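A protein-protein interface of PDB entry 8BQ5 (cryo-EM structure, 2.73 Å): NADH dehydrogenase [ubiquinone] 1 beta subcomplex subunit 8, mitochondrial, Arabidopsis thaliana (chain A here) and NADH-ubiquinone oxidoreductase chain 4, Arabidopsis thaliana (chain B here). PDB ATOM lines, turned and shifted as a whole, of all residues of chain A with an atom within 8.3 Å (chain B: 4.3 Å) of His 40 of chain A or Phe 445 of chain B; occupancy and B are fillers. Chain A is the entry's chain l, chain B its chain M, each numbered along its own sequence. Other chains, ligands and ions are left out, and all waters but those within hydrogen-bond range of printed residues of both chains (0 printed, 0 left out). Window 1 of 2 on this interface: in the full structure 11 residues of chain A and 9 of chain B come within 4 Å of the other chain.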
ATOM      1  N   VAL A  37       9.876 -15.912  -8.533  1.00  0.00           N
ATOM      2  CA  VAL A  37       9.790 -14.989  -7.409  1.00  0.00           C
ATOM      3  C   VAL A  37       9.306 -15.717  -6.163  1.00  0.00           C
ATOM      4  O   VAL A  37      10.105 -16.092  -5.305  1.00  0.00           O
ATOM      5  CB  VAL A  37       8.872 -13.797  -7.732  1.00  0.00           C
ATOM      6  CG1 VAL A  37       8.695 -12.913  -6.509  1.00  0.00           C
ATOM      7  CG2 VAL A  37       9.434 -12.994  -8.890  1.00  0.00           C
ATOM      8  N   GLY A  38       7.992 -15.923  -6.075  1.00  0.00           N
ATOM      9  CA  GLY A  38       7.394 -16.527  -4.903  1.00  0.00           C
ATOM     10  C   GLY A  38       7.906 -17.921  -4.616  1.00  0.00           C
ATOM     11  O   GLY A  38       8.270 -18.229  -3.477  1.00  0.00           O
ATOM     12  N   LYS A  39       7.942 -18.776  -5.637  1.00  0.00           N
ATOM     13  CA  LYS A  39       8.457 -20.130  -5.456  1.00  0.00           C
ATOM     14  C   LYS A  39       8.732 -20.719  -6.833  1.00  0.00           C
ATOM     15  O   LYS A  39       7.804 -20.880  -7.630  1.00  0.00           O
ATOM     16  CB  LYS A  39       7.462 -20.980  -4.672  1.00  0.00           C
ATOM     17  CG  LYS A  39       8.070 -22.167  -3.946  1.00  0.00           C
ATOM     18  CD  LYS A  39       8.004 -23.431  -4.775  1.00  0.00           C
ATOM     19  CE  LYS A  39       9.012 -24.459  -4.285  1.00  0.00           C
ATOM     20  NZ  LYS A  39       8.723 -25.818  -4.817  1.00  0.00           N
ATOM     21  N   HIS A  40       9.996 -21.030  -7.113  1.00  0.00           N
ATOM     22  CA  HIS A  40      10.323 -21.717  -8.354  1.00  0.00           C
ATOM     23  C   HIS A  40       9.909 -23.180  -8.256  1.00  0.00           C
ATOM     24  O   HIS A  40      10.020 -23.799  -7.194  1.00  0.00           O
ATOM     25  CB  HIS A  40      11.815 -21.594  -8.658  1.00  0.00           C
ATOM     26  CG  HIS A  40      12.688 -22.345  -7.704  1.00  0.00           C
ATOM     27  ND1 HIS A  40      13.287 -23.543  -8.030  1.00  0.00           N
ATOM     28  CD2 HIS A  40      13.056 -22.075  -6.430  1.00  0.00           C
ATOM     29  CE1 HIS A  40      13.992 -23.975  -6.999  1.00  0.00           C
ATOM     30  NE2 HIS A  40      13.868 -23.101  -6.016  1.00  0.00           N
ATOM     31  N   ILE A  41       9.429 -23.732  -9.369  1.00  0.00           N
ATOM     32  CA  ILE A  41       8.811 -25.051  -9.339  1.00  0.00           C
ATOM     33  C   ILE A  41       9.871 -26.117  -9.577  1.00  0.00           C
ATOM     34  O   ILE A  41      10.483 -26.185 -10.651  1.00  0.00           O
ATOM     35  CB  ILE A  41       7.671 -25.155 -10.368  1.00  0.00           C
ATOM     36  CG1 ILE A  41       6.669 -23.992 -10.253  1.00  0.00           C
ATOM     37  CG2 ILE A  41       6.928 -26.471 -10.202  1.00  0.00           C
ATOM     38  CD1 ILE A  41       7.096 -22.653 -10.854  1.00  0.00           C
ATOM     39  N   VAL A  42      10.096 -26.952  -8.569  1.00  0.00           N
ATOM     40  CA  VAL A  42      11.050 -28.052  -8.657  1.00  0.00           C
ATOM     41  C   VAL A  42      10.434 -29.138  -9.534  1.00  0.00           C
ATOM     42  O   VAL A  42       9.266 -29.499  -9.319  1.00  0.00           O
ATOM     43  CB  VAL A  42      11.402 -28.596  -7.266  1.00  0.00           C
ATOM     44  CG1 VAL A  42      12.192 -29.887  -7.375  1.00  0.00           C
ATOM     45  CG2 VAL A  42      12.190 -27.557  -6.488  1.00  0.00           C
ATOM     46  N   PRO A  43      11.151 -29.655 -10.531  1.00  0.00           N
ATOM     47  CA  PRO A  43      10.563 -30.680 -11.401  1.00  0.00           C
ATOM     48  C   PRO A  43      10.201 -31.940 -10.630  1.00  0.00           C
ATOM     49  O   PRO A  43      10.974 -32.438  -9.808  1.00  0.00           O
ATOM     50  CB  PRO A  43      11.666 -30.946 -12.431  1.00  0.00           C
ATOM     51  CG  PRO A  43      12.508 -29.719 -12.412  1.00  0.00           C
ATOM     52  CD  PRO A  43      12.488 -29.247 -10.989  1.00  0.00           C
ATOM     53  N   ARG B 365      20.674 -24.752 -15.210  1.00  0.00           N
ATOM     54  CA  ARG B 365      19.350 -24.604 -14.613  1.00  0.00           C
ATOM     55  C   ARG B 365      19.410 -24.450 -13.097  1.00  0.00           C
ATOM     56  O   ARG B 365      18.483 -23.896 -12.496  1.00  0.00           O
ATOM     57  CB  ARG B 365      18.469 -25.795 -14.987  1.00  0.00           C
ATOM     58  CG  ARG B 365      17.067 -25.700 -14.422  1.00  0.00           C
ATOM     59  CD  ARG B 365      16.195 -26.855 -14.867  1.00  0.00           C
ATOM     60  NE  ARG B 365      14.846 -26.724 -14.327  1.00  0.00           N
ATOM     61  CZ  ARG B 365      13.816 -27.474 -14.694  1.00  0.00           C
ATOM     62  NH1 ARG B 365      13.945 -28.432 -15.596  1.00  0.00           N
ATOM     63  NH2 ARG B 365      12.625 -27.251 -14.145  1.00  0.00           N
ATOM     64  N   TYR B 366      20.481 -24.927 -12.459  1.00  0.00           N
ATOM     65  CA  TYR B 366      20.581 -24.800 -11.008  1.00  0.00           C
ATOM     66  C   TYR B 366      20.864 -23.367 -10.577  1.00  0.00           C
ATOM     67  O   TYR B 366      20.467 -22.964  -9.478  1.00  0.00           O
ATOM     68  CB  TYR B 366      21.670 -25.724 -10.466  1.00  0.00           C
ATOM     69  CG  TYR B 366      21.272 -27.175 -10.383  1.00  0.00           C
ATOM     70  CD1 TYR B 366      20.109 -27.563  -9.733  1.00  0.00           C
ATOM     71  CD2 TYR B 366      22.069 -28.160 -10.943  1.00  0.00           C
ATOM     72  CE1 TYR B 366      19.750 -28.891  -9.651  1.00  0.00           C
ATOM     73  CE2 TYR B 366      21.720 -29.486 -10.868  1.00  0.00           C
ATOM     74  CZ  TYR B 366      20.562 -29.849 -10.221  1.00  0.00           C
ATOM     75  OH  TYR B 366      20.219 -31.176 -10.151  1.00  0.00           O
ATOM     76  N   LYS B 442      16.928 -19.425  -6.674  1.00  0.00           N
ATOM     77  CA  LYS B 442      16.178 -20.668  -6.520  1.00  0.00           C
ATOM     78  C   LYS B 442      16.643 -21.330  -5.228  1.00  0.00           C
ATOM     79  O   LYS B 442      17.530 -22.196  -5.241  1.00  0.00           O
ATOM     80  CB  LYS B 442      16.357 -21.580  -7.732  1.00  0.00           C
ATOM     81  CG  LYS B 442      15.995 -20.909  -9.045  1.00  0.00           C
ATOM     82  CD  LYS B 442      16.770 -21.483 -10.211  1.00  0.00           C
ATOM     83  CE  LYS B 442      16.313 -20.862 -11.519  1.00  0.00           C
ATOM     84  NZ  LYS B 442      17.008 -21.454 -12.692  1.00  0.00           N
ATOM     85  N   PRO B 443      16.064 -20.941  -4.088  1.00  0.00           N
ATOM     86  CA  PRO B 443      16.576 -21.426  -2.796  1.00  0.00           C
ATOM     87  C   PRO B 443      16.432 -22.924  -2.583  1.00  0.00           C
ATOM     88  O   PRO B 443      17.102 -23.467  -1.697  1.00  0.00           O
ATOM     89  CB  PRO B 443      15.756 -20.631  -1.770  1.00  0.00           C
ATOM     90  CG  PRO B 443      14.563 -20.138  -2.516  1.00  0.00           C
ATOM     91  CD  PRO B 443      15.009 -19.929  -3.925  1.00  0.00           C
ATOM     92  N   ASP B 444      15.579 -23.611  -3.346  1.00  0.00           N
ATOM     93  CA  ASP B 444      15.533 -25.064  -3.244  1.00  0.00           C
ATOM     94  C   ASP B 444      16.810 -25.715  -3.752  1.00  0.00           C
ATOM     95  O   ASP B 444      17.187 -26.782  -3.256  1.00  0.00           O
ATOM     96  CB  ASP B 444      14.332 -25.620  -4.007  1.00  0.00           C
ATOM     97  CG  ASP B 444      13.045 -25.511  -3.220  1.00  0.00           C
ATOM     98  OD1 ASP B 444      11.965 -25.696  -3.815  1.00  0.00           O
ATOM     99  OD2 ASP B 444      13.118 -25.240  -2.003  1.00  0.00           O
ATOM    100  N   PHE B 445      17.479 -25.105  -4.728  1.00  0.00           N
ATOM    101  CA  PHE B 445      18.749 -25.607  -5.236  1.00  0.00           C
ATOM    102  C   PHE B 445      19.942 -24.992  -4.516  1.00  0.00           C
ATOM    103  O   PHE B 445      20.847 -25.712  -4.089  1.00  0.00           O
ATOM    104  CB  PHE B 445      18.868 -25.338  -6.742  1.00  0.00           C
ATOM    105  CG  PHE B 445      17.711 -25.850  -7.547  1.00  0.00           C
ATOM    106  CD1 PHE B 445      17.146 -27.082  -7.272  1.00  0.00           C
ATOM    107  CD2 PHE B 445      17.203 -25.103  -8.597  1.00  0.00           C
ATOM    108  CE1 PHE B 445      16.085 -27.553  -8.020  1.00  0.00           C
ATOM    109  CE2 PHE B 445      16.146 -25.569  -9.347  1.00  0.00           C
ATOM    110  CZ  PHE B 445      15.586 -26.796  -9.057  1.00  0.00           C
ATOM    111  N   LEU B 446      19.962 -23.667  -4.379  1.00  0.00           N
ATOM    112  CA  LEU B 446      21.082 -22.962  -3.775  1.00  0.00           C
ATOM    113  C   LEU B 446      20.561 -21.869  -2.858  1.00  0.00           C
ATOM    114  O   LEU B 446      19.767 -21.025  -3.282  1.00  0.00           O
ATOM    115  CB  LEU B 446      21.999 -22.359  -4.847  1.00  0.00           C
ATOM    116  CG  LEU B 446      22.753 -23.352  -5.730  1.00  0.00           C
ATOM    117  CD1 LEU B 446      23.244 -22.693  -7.004  1.00  0.00           C
ATOM    118  CD2 LEU B 446      23.911 -23.942  -4.951  1.00  0.00           C
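Hydrophobic or aromatic side chains of chain B within 4 Å of the printed part of chain A: Pro 443 and Phe 445. Among the printed residues, 7 pairs touch across the chains. Among the printed residues, Asp or Glu carboxylates within 4 Å of a Lys or Arg side-chain nitrogen of the other chain: Lys 39 of chain A with Asp 444 of chain B.
Of chain B, only Lys 442 (3.4 Å), Pro 443 (3.6 Å), Asp 444 (3.2 Å) and Phe 445 (3.6 Å) come within 4 Å of His 40 of chain A. Phe 445 of chain B touches just one residue of chain A: His 40. Printed residues of chain B within 4 Å of Val 42 of chain A: Asp 444. Printed residues of chain A within 4 Å of Arg 365 of chain B: Pro 43 (3.0 Å). Val 37 of chain A touches none of the printed residues of chain B. The nearest residue of chain A that does not touch Phe 445 of chain B is Val 42 of chain A (4.2 Å).
His 40 of chain A touches Lys 442 of chain B (NE2 to CB, 3.4 Å). His 40 of chain A touches Pro 443 of chain B. His 40 of chain A touches Phe 445 of chain B. CG2 of Val 42 of chain A touches OD1 of Asp 444 of chain B, 3.3 Å away. Pro 43 of chain A touches Arg 365 of chain B (CG to NH2, 3.0 Å).
O of Arg 365 of chain B sits at hydrogen-bond distance from NZ of Lys 442 of chain B.
The side-chain amino group of Lys 39 of chain A is in salt-bridge range of the side-chain carboxylate of Asp 444 of chain B. A ring nitrogen (NE2) of His 40 of chain A is in hydrogen-bond range of the backbone NH (N) of Asp 444 of chain B (3.2 Å).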
